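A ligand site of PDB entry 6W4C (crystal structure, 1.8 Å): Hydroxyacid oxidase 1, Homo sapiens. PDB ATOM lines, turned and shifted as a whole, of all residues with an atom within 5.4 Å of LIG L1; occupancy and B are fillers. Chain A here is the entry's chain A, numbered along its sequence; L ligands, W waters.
NH1 of Arg 315 is in salt-bridge range of O8 of LIG L1, 3.0 Å away. N2 of LIG L1 sits close to NE2 of Gln 130, 3.0 Å away. The backbone NH of Ala 81 lies within hydrogen-bond range of a nitrogen (N3) of LIG L1. O2 of LG2 L2 sits at hydrogen-bond distance from OH of Tyr 26 (2.7 Å). N of Gly 314 sits at hydrogen-bond distance from O7 of LIG L1, 2.9 Å away. The guanidinium group (NH2) of Arg 295 is in salt-bridge range of an oxygen (O9) of LIG L1 (2.7 Å). O1 of LIG L1 lies within hydrogen-bond range of OG1 of Thr 158 (2.7 Å). A nitrogen (N1) of LG2 L2 is in hydrogen-bond range of a ring nitrogen (NE2) of His 260, 2.8 Å away. The side-chain hydroxyl of Tyr 132 lies within hydrogen-bond range of a nitrogen (N2) of LIG L1 (3.4 Å). OD2 of Asp 291 sits at hydrogen-bond distance from O4 of LIG L1 (2.8 Å). An oxygen (O8) of LIG L1 is in hydrogen-bond range of the backbone NH (N) of Arg 315 (3.0 Å). OG of Ser 108 lies within hydrogen-bond range of O2 of LIG L1 (2.7 Å). The backbone carbonyl oxygen (O) of Ala 79 is in hydrogen-bond range of an oxygen (O3) of LIG L1, 2.6 Å away. OG of Ser 258 is in hydrogen-bond range of O4 of LIG L1. NZ of Lys 236 sits at hydrogen-bond distance from O1 of LIG L1, 2.9 Å away. A nitrogen (N2) of LG2 L2 sits at hydrogen-bond distance from the side-chain hydroxyl (OH) of Tyr 132 (2.6 Å). The backbone NH (N) of Gly 293 sits at hydrogen-bond distance from an oxygen (O9) of LIG L1. The guanidinium group (NE) of Arg 263 is in salt-bridge range of an oxygen (O1) of LG2 L2, 2.8 Å away.
A nitrogen (N1) of LG2 L2 sits close to a nitrogen (N3) of LIG L1.
The side-chain hydroxyl (OG1) of Thr 158 lies within hydrogen-bond range of the side-chain amide oxygen (OE1) of Gln 130, 3.0 Å away. The side-chain hydroxyl of Ser 108 is in hydrogen-bond range of the backbone NH of Trp 110 (3.0 Å). The side-chain hydroxyl (OG) of Ser 258 is in hydrogen-bond range of the side-chain carboxylate (OD1) of Asp 291, at 2.6 Å. The guanidinium group of Arg 315 is in hydrogen-bond range of the backbone carbonyl oxygen of Tyr 27, at 2.9 Å. The backbone NH (N) of Ala 79 sits close to the backbone carbonyl oxygen (O) of Met 106, 3.5 Å away. The side-chain amide nitrogen (NE2) of Gln 130 lies close to the backbone NH (N) of Ser 109, at 3.1 Å. O of Tyr 27 lies within hydrogen-bond range of NH1 of Arg 263, at 3.3 Å. The side-chain hydroxyl of Ser 258 is in hydrogen-bond range of the backbone NH of His 260, at 3.0 Å.
Residues that only touch LIG L1: Gly 261 (3.4 Å), Arg 263 (3.5 Å), Gly 292 (3.5 Å), His 260 (3.5 Å), Thr 80 (3.5 Å), Tyr 27 (3.6 Å), Tyr 26 (3.7 Å), Val 313 (3.8 Å) and Pro 316 (3.998 Å). Hydrophobic or aromatic side chains within 4 Å of LIG L1: Tyr 26, Tyr 27, Ala 81, Tyr 132, His 260 and Pro 316.
Water W2 lies within hydrogen-bond range of O9 of LIG L1, ND2 of Asn 40, NH1 of Arg 315 and O of Gly 261. Water W1 lies within hydrogen-bond range of the side-chain carboxylate (OD2) of Asp 291 (2.7 Å) and an oxygen (O3) of LIG L1 (3.0 Å).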
ATOM      1  N   TYR A  26      20.033 -29.875  28.398  1.00  0.00           N
ATOM      2  CA  TYR A  26      19.713 -29.255  27.085  1.00  0.00           C
ATOM      3  C   TYR A  26      20.805 -29.651  26.071  1.00  0.00           C
ATOM      4  O   TYR A  26      20.468 -30.086  24.933  1.00  0.00           O
ATOM      5  CB  TYR A  26      19.588 -27.739  27.149  1.00  0.00           C
ATOM      6  CG  TYR A  26      19.672 -27.103  25.783  1.00  0.00           C
ATOM      7  CD1 TYR A  26      18.641 -27.271  24.867  1.00  0.00           C
ATOM      8  CD2 TYR A  26      20.785 -26.398  25.375  1.00  0.00           C
ATOM      9  CE1 TYR A  26      18.716 -26.733  23.594  1.00  0.00           C
ATOM     10  CE2 TYR A  26      20.866 -25.844  24.108  1.00  0.00           C
ATOM     11  CZ  TYR A  26      19.845 -26.037  23.209  1.00  0.00           C
ATOM     12  OH  TYR A  26      19.928 -25.514  21.951  1.00  0.00           O
ATOM     13  N   TYR A  27      22.067 -29.528  26.465  1.00  0.00           N
ATOM     14  CA  TYR A  27      23.215 -29.802  25.560  1.00  0.00           C
ATOM     15  C   TYR A  27      23.329 -31.301  25.272  1.00  0.00           C
ATOM     16  O   TYR A  27      23.613 -31.664  24.103  1.00  0.00           O
ATOM     17  CB  TYR A  27      24.516 -29.289  26.169  1.00  0.00           C
ATOM     18  CG  TYR A  27      24.669 -27.786  26.202  1.00  0.00           C
ATOM     19  CD1 TYR A  27      24.369 -26.994  25.108  1.00  0.00           C
ATOM     20  CD2 TYR A  27      25.184 -27.165  27.322  1.00  0.00           C
ATOM     21  CE1 TYR A  27      24.553 -25.617  25.125  1.00  0.00           C
ATOM     22  CE2 TYR A  27      25.372 -25.791  27.362  1.00  0.00           C
ATOM     23  CZ  TYR A  27      25.057 -25.020  26.254  1.00  0.00           C
ATOM     24  OH  TYR A  27      25.251 -23.668  26.289  1.00  0.00           O
ATOM     25  N   ASN A  40      24.857 -43.059  17.369  1.00  0.00           N
ATOM     26  CA  ASN A  40      25.864 -42.173  16.699  1.00  0.00           C
ATOM     27  C   ASN A  40      27.279 -42.521  17.181  1.00  0.00           C
ATOM     28  O   ASN A  40      28.216 -42.497  16.356  1.00  0.00           O
ATOM     29  CB  ASN A  40      25.598 -40.683  16.929  1.00  0.00           C
ATOM     30  CG  ASN A  40      24.600 -40.114  15.944  1.00  0.00           C
ATOM     31  OD1 ASN A  40      24.182 -40.799  15.009  1.00  0.00           O
ATOM     32  ND2 ASN A  40      24.204 -38.863  16.176  1.00  0.00           N
ATOM     33  N   GLY A  78      30.848 -27.360  14.297  1.00  0.00           N
ATOM     34  CA  GLY A  78      29.446 -27.347  13.832  1.00  0.00           C
ATOM     35  C   GLY A  78      28.632 -26.314  14.575  1.00  0.00           C
ATOM     36  O   GLY A  78      29.033 -25.916  15.692  1.00  0.00           O
ATOM     37  N   ALA A  79      27.497 -25.940  14.007  1.00  0.00           N
ATOM     38  CA  ALA A  79      26.567 -24.938  14.573  1.00  0.00           C
ATOM     39  C   ALA A  79      25.947 -25.469  15.862  1.00  0.00           C
ATOM     40  O   ALA A  79      25.392 -26.575  15.851  1.00  0.00           O
ATOM     41  CB  ALA A  79      25.511 -24.618  13.539  1.00  0.00           C
ATOM     42  N   THR A  80      26.035 -24.732  16.953  1.00  0.00           N
ATOM     43  CA  THR A  80      25.311 -25.036  18.206  1.00  0.00           C
ATOM     44  C   THR A  80      24.745 -23.722  18.714  1.00  0.00           C
ATOM     45  O   THR A  80      25.535 -22.779  18.886  1.00  0.00           O
ATOM     46  CB  THR A  80      26.168 -25.765  19.241  1.00  0.00           C
ATOM     47  OG1 THR A  80      27.368 -25.014  19.435  1.00  0.00           O
ATOM     48  CG2 THR A  80      26.517 -27.185  18.842  1.00  0.00           C
ATOM     49  N   ALA A  81      23.416 -23.633  18.821  1.00  0.00           N
ATOM     50  CA  ALA A  81      22.681 -22.406  19.179  1.00  0.00           C
ATOM     51  C   ALA A  81      23.151 -21.904  20.556  1.00  0.00           C
ATOM     52  O   ALA A  81      23.492 -22.744  21.403  1.00  0.00           O
ATOM     53  CB  ALA A  81      21.201 -22.684  19.181  1.00  0.00           C
ATOM     54  N   MET A 106      31.249 -23.110  11.744  1.00  0.00           N
ATOM     55  CA  MET A 106      29.859 -22.943  11.295  1.00  0.00           C
ATOM     56  C   MET A 106      29.093 -22.224  12.415  1.00  0.00           C
ATOM     57  O   MET A 106      28.926 -22.811  13.495  1.00  0.00           O
ATOM     58  CB  MET A 106      29.226 -24.313  11.020  1.00  0.00           C
ATOM     59  CG  MET A 106      27.984 -24.255  10.164  1.00  0.00           C
ATOM     60  SD  MET A 106      27.007 -25.763  10.354  1.00  0.00           S
ATOM     61  CE  MET A 106      28.149 -27.010   9.776  1.00  0.00           C
ATOM     62  N   SER A 108      25.761 -20.818  14.105  1.00  0.00           N
ATOM     63  CA  SER A 108      24.299 -21.033  14.181  1.00  0.00           C
ATOM     64  C   SER A 108      23.578 -19.746  13.758  1.00  0.00           C
ATOM     65  O   SER A 108      24.059 -18.676  14.116  1.00  0.00           O
ATOM     66  CB  SER A 108      23.916 -21.444  15.566  1.00  0.00           C
ATOM     67  OG  SER A 108      22.509 -21.484  15.713  1.00  0.00           O
ATOM     68  N   SER A 109      22.474 -19.804  13.007  1.00  0.00           N
ATOM     69  CA  SER A 109      21.719 -18.549  12.741  1.00  0.00           C
ATOM     70  C   SER A 109      20.877 -18.211  13.989  1.00  0.00           C
ATOM     71  O   SER A 109      20.287 -17.121  14.000  1.00  0.00           O
ATOM     72  CB  SER A 109      20.885 -18.577  11.486  1.00  0.00           C
ATOM     73  OG  SER A 109      19.982 -19.652  11.502  1.00  0.00           O
ATOM     74  N   TRP A 110      20.893 -19.067  15.012  1.00  0.00           N
ATOM     75  CA  TRP A 110      20.306 -18.728  16.339  1.00  0.00           C
ATOM     76  C   TRP A 110      21.429 -18.565  17.381  1.00  0.00           C
ATOM     77  O   TRP A 110      21.424 -19.276  18.392  1.00  0.00           O
ATOM     78  CB  TRP A 110      19.239 -19.752  16.739  1.00  0.00           C
ATOM     79  CG  TRP A 110      18.182 -19.118  17.575  1.00  0.00           C
ATOM     80  CD1 TRP A 110      18.271 -18.769  18.889  1.00  0.00           C
ATOM     81  CD2 TRP A 110      16.883 -18.690  17.139  1.00  0.00           C
ATOM     82  NE1 TRP A 110      17.105 -18.178  19.312  1.00  0.00           N
ATOM     83  CE2 TRP A 110      16.238 -18.103  18.256  1.00  0.00           C
ATOM     84  CE3 TRP A 110      16.193 -18.750  15.924  1.00  0.00           C
ATOM     85  CZ2 TRP A 110      14.945 -17.597  18.184  1.00  0.00           C
ATOM     86  CZ3 TRP A 110      14.910 -18.241  15.850  1.00  0.00           C
ATOM     87  CH2 TRP A 110      14.291 -17.666  16.970  1.00  0.00           C
ATOM     88  N   GLN A 130      25.321 -21.176   9.224  1.00  0.00           N
ATOM     89  CA  GLN A 130      24.190 -22.116   9.243  1.00  0.00           C
ATOM     90  C   GLN A 130      22.920 -21.280   9.164  1.00  0.00           C
ATOM     91  O   GLN A 130      22.795 -20.294   9.911  1.00  0.00           O
ATOM     92  CB  GLN A 130      24.188 -23.002  10.485  1.00  0.00           C
ATOM     93  CG  GLN A 130      23.024 -23.990  10.530  1.00  0.00           C
ATOM     94  CD  GLN A 130      21.765 -23.431  11.152  1.00  0.00           C
ATOM     95  OE1 GLN A 130      20.650 -23.592  10.632  1.00  0.00           O
ATOM     96  NE2 GLN A 130      21.929 -22.804  12.297  1.00  0.00           N
ATOM     97  N   TYR A 132      18.533 -21.415   8.798  1.00  0.00           N
ATOM     98  CA  TYR A 132      17.151 -21.930   8.661  1.00  0.00           C
ATOM     99  C   TYR A 132      16.436 -21.008   7.680  1.00  0.00           C
ATOM    100  O   TYR A 132      16.682 -19.787   7.765  1.00  0.00           O
ATOM    101  CB  TYR A 132      16.412 -21.949   9.994  1.00  0.00           C
ATOM    102  CG  TYR A 132      16.912 -22.994  10.953  1.00  0.00           C
ATOM    103  CD1 TYR A 132      16.674 -24.330  10.694  1.00  0.00           C
ATOM    104  CD2 TYR A 132      17.593 -22.656  12.105  1.00  0.00           C
ATOM    105  CE1 TYR A 132      17.110 -25.316  11.562  1.00  0.00           C
ATOM    106  CE2 TYR A 132      18.048 -23.629  12.990  1.00  0.00           C
ATOM    107  CZ  TYR A 132      17.806 -24.962  12.709  1.00  0.00           C
ATOM    108  OH  TYR A 132      18.229 -25.950  13.547  1.00  0.00           O
ATOM    109  N   THR A 158      20.004 -25.915   6.957  1.00  0.00           N
ATOM    110  CA  THR A 158      19.531 -27.076   7.735  1.00  0.00           C
ATOM    111  C   THR A 158      18.169 -27.486   7.179  1.00  0.00           C
ATOM    112  O   THR A 158      17.279 -26.633   7.120  1.00  0.00           O
ATOM    113  CB  THR A 158      19.496 -26.765   9.230  1.00  0.00           C
ATOM    114  OG1 THR A 158      20.826 -26.438   9.624  1.00  0.00           O
ATOM    115  CG2 THR A 158      18.973 -27.924  10.039  1.00  0.00           C
ATOM    116  N   LYS A 236      22.395 -29.525   4.979  1.00  0.00           N
ATOM    117  CA  LYS A 236      22.727 -30.114   6.303  1.00  0.00           C
ATOM    118  C   LYS A 236      21.518 -30.901   6.821  1.00  0.00           C
ATOM    119  O   LYS A 236      20.467 -30.269   7.083  1.00  0.00           O
ATOM    120  CB  LYS A 236      23.122 -28.990   7.252  1.00  0.00           C
ATOM    121  CG  LYS A 236      23.379 -29.417   8.695  1.00  0.00           C
ATOM    122  CD  LYS A 236      23.850 -28.272   9.542  1.00  0.00           C
ATOM    123  CE  LYS A 236      24.312 -28.695  10.918  1.00  0.00           C
ATOM    124  NZ  LYS A 236      23.172 -29.035  11.801  1.00  0.00           N
ATOM    125  N   SER A 258      23.922 -35.738   8.498  1.00  0.00           N
ATOM    126  CA  SER A 258      23.678 -35.262   9.883  1.00  0.00           C
ATOM    127  C   SER A 258      22.294 -35.739  10.288  1.00  0.00           C
ATOM    128  O   SER A 258      21.392 -35.739   9.433  1.00  0.00           O
ATOM    129  CB  SER A 258      23.788 -33.771   9.971  1.00  0.00           C
ATOM    130  OG  SER A 258      23.454 -33.308  11.278  1.00  0.00           O
ATOM    131  N   HIS A 260      21.319 -34.212  13.151  1.00  0.00           N
ATOM    132  CA  HIS A 260      21.159 -33.063  14.079  1.00  0.00           C
ATOM    133  C   HIS A 260      21.596 -33.499  15.481  1.00  0.00           C
ATOM    134  O   HIS A 260      20.909 -33.148  16.461  1.00  0.00           O
ATOM    135  CB  HIS A 260      19.700 -32.580  14.068  1.00  0.00           C
ATOM    136  CG  HIS A 260      19.511 -31.147  14.419  1.00  0.00           C
ATOM    137  ND1 HIS A 260      19.088 -30.221  13.485  1.00  0.00           N
ATOM    138  CD2 HIS A 260      19.649 -30.466  15.590  1.00  0.00           C
ATOM    139  CE1 HIS A 260      18.969 -29.036  14.067  1.00  0.00           C
ATOM    140  NE2 HIS A 260      19.308 -29.166  15.357  1.00  0.00           N
ATOM    141  N   GLY A 261      22.653 -34.301  15.574  1.00  0.00           N
ATOM    142  CA  GLY A 261      23.146 -34.813  16.872  1.00  0.00           C
ATOM    143  C   GLY A 261      22.094 -35.653  17.571  1.00  0.00           C
ATOM    144  O   GLY A 261      22.065 -35.656  18.827  1.00  0.00           O
ATOM    145  N   ARG A 263      18.876 -35.222  17.748  1.00  0.00           N
ATOM    146  CA  ARG A 263      17.947 -34.342  18.497  1.00  0.00           C
ATOM    147  C   ARG A 263      16.625 -34.137  17.754  1.00  0.00           C
ATOM    148  O   ARG A 263      15.731 -33.457  18.312  1.00  0.00           O
ATOM    149  CB  ARG A 263      18.653 -33.010  18.740  1.00  0.00           C
ATOM    150  CG  ARG A 263      19.862 -33.141  19.652  1.00  0.00           C
ATOM    151  CD  ARG A 263      20.746 -31.921  19.623  1.00  0.00           C
ATOM    152  NE  ARG A 263      20.199 -30.736  20.274  1.00  0.00           N
ATOM    153  CZ  ARG A 263      20.288 -30.477  21.585  1.00  0.00           C
ATOM    154  NH1 ARG A 263      20.790 -31.358  22.420  1.00  0.00           N
ATOM    155  NH2 ARG A 263      19.830 -29.333  22.058  1.00  0.00           N
ATOM    156  N   ASP A 291      28.570 -35.191  10.543  1.00  0.00           N
ATOM    157  CA  ASP A 291      28.581 -34.876  11.994  1.00  0.00           C
ATOM    158  C   ASP A 291      27.731 -35.922  12.711  1.00  0.00           C
ATOM    159  O   ASP A 291      27.029 -36.679  12.042  1.00  0.00           O
ATOM    160  CB  ASP A 291      28.197 -33.423  12.290  1.00  0.00           C
ATOM    161  CG  ASP A 291      26.740 -33.046  12.071  1.00  0.00           C
ATOM    162  OD1 ASP A 291      25.868 -33.949  12.138  1.00  0.00           O
ATOM    163  OD2 ASP A 291      26.490 -31.844  11.876  1.00  0.00           O
ATOM    164  N   GLY A 292      27.821 -35.971  14.032  1.00  0.00           N
ATOM    165  CA  GLY A 292      27.053 -36.910  14.851  1.00  0.00           C
ATOM    166  C   GLY A 292      27.956 -37.953  15.448  1.00  0.00           C
ATOM    167  O   GLY A 292      28.306 -38.923  14.766  1.00  0.00           O
ATOM    168  N   GLY A 293      28.348 -37.762  16.701  1.00  0.00           N
ATOM    169  CA  GLY A 293      29.037 -38.806  17.459  1.00  0.00           C
ATOM    170  C   GLY A 293      30.545 -38.746  17.325  1.00  0.00           C
ATOM    171  O   GLY A 293      31.190 -39.654  17.852  1.00  0.00           O
ATOM    172  N   VAL A 294      31.106 -37.739  16.665  1.00  0.00           N
ATOM    173  CA  VAL A 294      32.588 -37.631  16.538  1.00  0.00           C
ATOM    174  C   VAL A 294      33.167 -37.207  17.885  1.00  0.00           C
ATOM    175  O   VAL A 294      32.867 -36.095  18.345  1.00  0.00           O
ATOM    176  CB  VAL A 294      33.011 -36.697  15.401  1.00  0.00           C
ATOM    177  CG1 VAL A 294      34.510 -36.536  15.393  1.00  0.00           C
ATOM    178  CG2 VAL A 294      32.491 -37.195  14.065  1.00  0.00           C
ATOM    179  N   ARG A 295      33.977 -38.069  18.501  1.00  0.00           N
ATOM    180  CA  ARG A 295      34.554 -37.820  19.860  1.00  0.00           C
ATOM    181  C   ARG A 295      36.044 -38.142  19.884  1.00  0.00           C
ATOM    182  O   ARG A 295      36.694 -37.748  20.853  1.00  0.00           O
ATOM    183  CB  ARG A 295      33.846 -38.667  20.912  1.00  0.00           C
ATOM    184  CG  ARG A 295      32.349 -38.464  21.018  1.00  0.00           C
ATOM    185  CD  ARG A 295      31.932 -37.111  21.543  1.00  0.00           C
ATOM    186  NE  ARG A 295      30.470 -36.970  21.583  1.00  0.00           N
ATOM    187  CZ  ARG A 295      29.723 -36.407  20.628  1.00  0.00           C
ATOM    188  NH1 ARG A 295      30.288 -35.892  19.544  1.00  0.00           N
ATOM    189  NH2 ARG A 295      28.409 -36.342  20.784  1.00  0.00           N
ATOM    190  N   PHE A 312      32.310 -32.496  11.342  1.00  0.00           N
ATOM    191  CA  PHE A 312      31.957 -31.384  12.243  1.00  0.00           C
ATOM    192  C   PHE A 312      31.683 -31.955  13.623  1.00  0.00           C
ATOM    193  O   PHE A 312      31.182 -33.082  13.732  1.00  0.00           O
ATOM    194  CB  PHE A 312      30.768 -30.596  11.717  1.00  0.00           C
ATOM    195  CG  PHE A 312      31.054 -29.868  10.436  1.00  0.00           C
ATOM    196  CD1 PHE A 312      31.057 -30.542   9.219  1.00  0.00           C
ATOM    197  CD2 PHE A 312      31.375 -28.521  10.440  1.00  0.00           C
ATOM    198  CE1 PHE A 312      31.343 -29.872   8.039  1.00  0.00           C
ATOM    199  CE2 PHE A 312      31.652 -27.858   9.252  1.00  0.00           C
ATOM    200  CZ  PHE A 312      31.636 -28.532   8.056  1.00  0.00           C
ATOM    201  N   VAL A 313      32.018 -31.187  14.649  1.00  0.00           N
ATOM    202  CA  VAL A 313      31.752 -31.554  16.071  1.00  0.00           C
ATOM    203  C   VAL A 313      30.833 -30.488  16.649  1.00  0.00           C
ATOM    204  O   VAL A 313      31.070 -29.291  16.407  1.00  0.00           O
ATOM    205  CB  VAL A 313      33.045 -31.715  16.886  1.00  0.00           C
ATOM    206  CG1 VAL A 313      33.714 -33.040  16.579  1.00  0.00           C
ATOM    207  CG2 VAL A 313      34.015 -30.555  16.696  1.00  0.00           C
ATOM    208  N   GLY A 314      29.767 -30.932  17.311  1.00  0.00           N
ATOM    209  CA  GLY A 314      28.839 -30.041  18.026  1.00  0.00           C
ATOM    210  C   GLY A 314      29.128 -30.020  19.510  1.00  0.00           C
ATOM    211  O   GLY A 314      29.786 -29.081  19.989  1.00  0.00           O
ATOM    212  N   ARG A 315      28.694 -31.041  20.224  1.00  0.00           N
ATOM    213  CA  ARG A 315      28.718 -31.057  21.703  1.00  0.00           C
ATOM    214  C   ARG A 315      30.136 -30.878  22.234  1.00  0.00           C
ATOM    215  O   ARG A 315      30.292 -30.155  23.224  1.00  0.00           O
ATOM    216  CB  ARG A 315      28.059 -32.311  22.260  1.00  0.00           C
ATOM    217  CG  ARG A 315      26.543 -32.289  22.119  1.00  0.00           C
ATOM    218  CD  ARG A 315      25.966 -33.579  22.634  1.00  0.00           C
ATOM    219  NE  ARG A 315      24.550 -33.732  22.377  1.00  0.00           N
ATOM    220  CZ  ARG A 315      23.995 -34.258  21.291  1.00  0.00           C
ATOM    221  NH1 ARG A 315      24.737 -34.608  20.247  1.00  0.00           N
ATOM    222  NH2 ARG A 315      22.678 -34.383  21.222  1.00  0.00           N
ATOM    223  N   PRO A 316      31.193 -31.508  21.668  1.00  0.00           N
ATOM    224  CA  PRO A 316      32.542 -31.340  22.214  1.00  0.00           C
ATOM    225  C   PRO A 316      32.933 -29.866  22.367  1.00  0.00           C
ATOM    226  O   PRO A 316      33.626 -29.531  23.342  1.00  0.00           O
ATOM    227  CB  PRO A 316      33.428 -32.087  21.216  1.00  0.00           C
ATOM    228  CG  PRO A 316      32.503 -33.206  20.744  1.00  0.00           C
ATOM    229  CD  PRO A 316      31.172 -32.501  20.570  1.00  0.00           C
ATOM    230  N   VAL A 318      30.909 -27.244  22.947  1.00  0.00           N
ATOM    231  CA  VAL A 318      30.146 -26.703  24.100  1.00  0.00           C
ATOM    232  C   VAL A 318      30.846 -27.135  25.403  1.00  0.00           C
ATOM    233  O   VAL A 318      30.966 -26.302  26.329  1.00  0.00           O
ATOM    234  CB  VAL A 318      28.682 -27.161  24.072  1.00  0.00           C
ATOM    235  CG1 VAL A 318      27.969 -26.753  25.349  1.00  0.00           C
ATOM    236  CG2 VAL A 318      27.970 -26.613  22.839  1.00  0.00           C
HETATM  237  N1  LIG L   1      22.223 -27.487  14.146  1.00  0.00           N
HETATM  238  C1  LIG L   1      21.848 -26.420  13.398  1.00  0.00           C
HETATM  239  O1  LIG L   1      21.785 -26.552  12.143  1.00  0.00           O
HETATM  240  N2  LIG L   1      21.561 -25.218  13.956  1.00  0.00           N
HETATM  241  C2  LIG L   1      21.617 -25.015  15.274  1.00  0.00           C
HETATM  242  O2  LIG L   1      21.345 -23.930  15.794  1.00  0.00           O
HETATM  243  C3  LIG L   1      21.983 -26.138  16.143  1.00  0.00           C
HETATM  244  N3  LIG L   1      22.025 -26.010  17.483  1.00  0.00           N
HETATM  245  C4  LIG L   1      22.419 -27.035  18.239  1.00  0.00           C
HETATM  246  C5  LIG L   1      22.508 -26.877  19.621  1.00  0.00           C
HETATM  247  C6  LIG L   1      22.916 -27.937  20.388  1.00  0.00           C
HETATM  248  C7  LIG L   1      23.008 -27.780  21.875  1.00  0.00           C
HETATM  249  C8  LIG L   1      23.277 -29.240  19.806  1.00  0.00           C
HETATM  250  C9  LIG L   1      23.740 -30.391  20.683  1.00  0.00           C
HETATM  251  C10 LIG L   1      23.213 -29.409  18.427  1.00  0.00           C
HETATM  252  C11 LIG L   1      22.786 -28.334  17.625  1.00  0.00           C
HETATM  253  N4  LIG L   1      22.705 -28.489  16.241  1.00  0.00           N
HETATM  254  C12 LIG L   1      22.329 -27.397  15.465  1.00  0.00           C
HETATM  255  C13 LIG L   1      23.085 -29.723  15.566  1.00  0.00           C
HETATM  256  C14 LIG L   1      24.600 -29.611  15.374  1.00  0.00           C
HETATM  257  O3  LIG L   1      24.937 -28.662  14.359  1.00  0.00           O
HETATM  258  C15 LIG L   1      25.260 -30.920  14.947  1.00  0.00           C
HETATM  259  O4  LIG L   1      24.533 -31.538  13.849  1.00  0.00           O
HETATM  260  C16 LIG L   1      25.360 -31.923  16.077  1.00  0.00           C
HETATM  261  O5  LIG L   1      25.701 -31.308  17.327  1.00  0.00           O
HETATM  262  C17 LIG L   1      26.417 -32.961  15.750  1.00  0.00           C
HETATM  263  O6  LIG L   1      26.486 -34.035  16.682  1.00  0.00           O
HETATM  264  P1  LIG L   1      27.503 -34.102  17.942  1.00  0.00           P
HETATM  265  O7  LIG L   1      28.880 -33.650  17.502  1.00  0.00           O
HETATM  266  O8  LIG L   1      26.944 -33.127  18.950  1.00  0.00           O
HETATM  267  O9  LIG L   1      27.397 -35.546  18.383  1.00  0.00           O
HETATM  268  C1  LG2 L   2      18.780 -23.943  27.940  1.00  0.00           C
HETATM  269  C2  LG2 L   2      16.658 -25.058  27.452  1.00  0.00           C
HETATM  270  C3  LG2 L   2      15.891 -25.004  25.565  1.00  0.00           C
HETATM  271  C4  LG2 L   2      15.430 -23.958  21.470  1.00  0.00           C
HETATM  272  C5  LG2 L   2      16.519 -23.471  22.184  1.00  0.00           C
HETATM  273  C6  LG2 L   2      17.571 -22.567  21.591  1.00  0.00           C
HETATM  274  C7  LG2 L   2      17.665 -23.040  19.141  1.00  0.00           C
HETATM  275  C8  LG2 L   2      18.048 -24.375  19.353  1.00  0.00           C
HETATM  276  C9  LG2 L   2      18.313 -25.182  18.247  1.00  0.00           C
HETATM  277  C10 LG2 L   2      18.183 -24.640  16.954  1.00  0.00           C
HETATM  278  C11 LG2 L   2      18.687 -26.549  18.030  1.00  0.00           C
HETATM  279  C12 LG2 L   2      18.938 -27.646  18.987  1.00  0.00           C
HETATM  280  C13 LG2 L   2      17.816 -23.319  16.746  1.00  0.00           C
HETATM  281  O1  LG2 L   2      19.167 -28.781  18.576  1.00  0.00           O
HETATM  282  O2  LG2 L   2      18.886 -27.333  20.251  1.00  0.00           O
HETATM  283  N1  LG2 L   2      18.783 -26.812  16.728  1.00  0.00           N
HETATM  284  N2  LG2 L   2      18.470 -25.645  16.085  1.00  0.00           N
HETATM  285  C14 LG2 L   2      17.549 -22.536  17.850  1.00  0.00           C
HETATM  286  N3  LG2 L   2      17.383 -22.196  20.206  1.00  0.00           N
HETATM  287  C15 LG2 L   2      14.505 -24.802  22.064  1.00  0.00           C
HETATM  288  C16 LG2 L   2      14.639 -25.188  23.392  1.00  0.00           C
HETATM  289  C17 LG2 L   2      16.649 -23.845  23.519  1.00  0.00           C
HETATM  290  O3  LG2 L   2      17.715 -23.371  24.185  1.00  0.00           O
HETATM  291  C18 LG2 L   2      15.709 -24.699  24.137  1.00  0.00           C
HETATM  292  O4  LG2 L   2      15.121 -25.857  26.264  1.00  0.00           O
HETATM  293  N4  LG2 L   2      15.660 -25.878  27.590  1.00  0.00           N
HETATM  294  N5  LG2 L   2      16.849 -24.484  26.261  1.00  0.00           N
HETATM  295  N6  LG2 L   2      17.599 -24.698  28.343  1.00  0.00           N
HETATM  296  C19 LG2 L   2      17.515 -25.042  29.756  1.00  0.00           C
HETATM  297  O   HOH W   1      27.229 -29.293  12.543  1.00  0.00           O
HETATM  298  O   HOH W   2      25.152 -37.079  18.327  1.00  0.00           O
HETATM  299  O   HOH W   3      29.992 -34.969  15.494  1.00  0.00           O
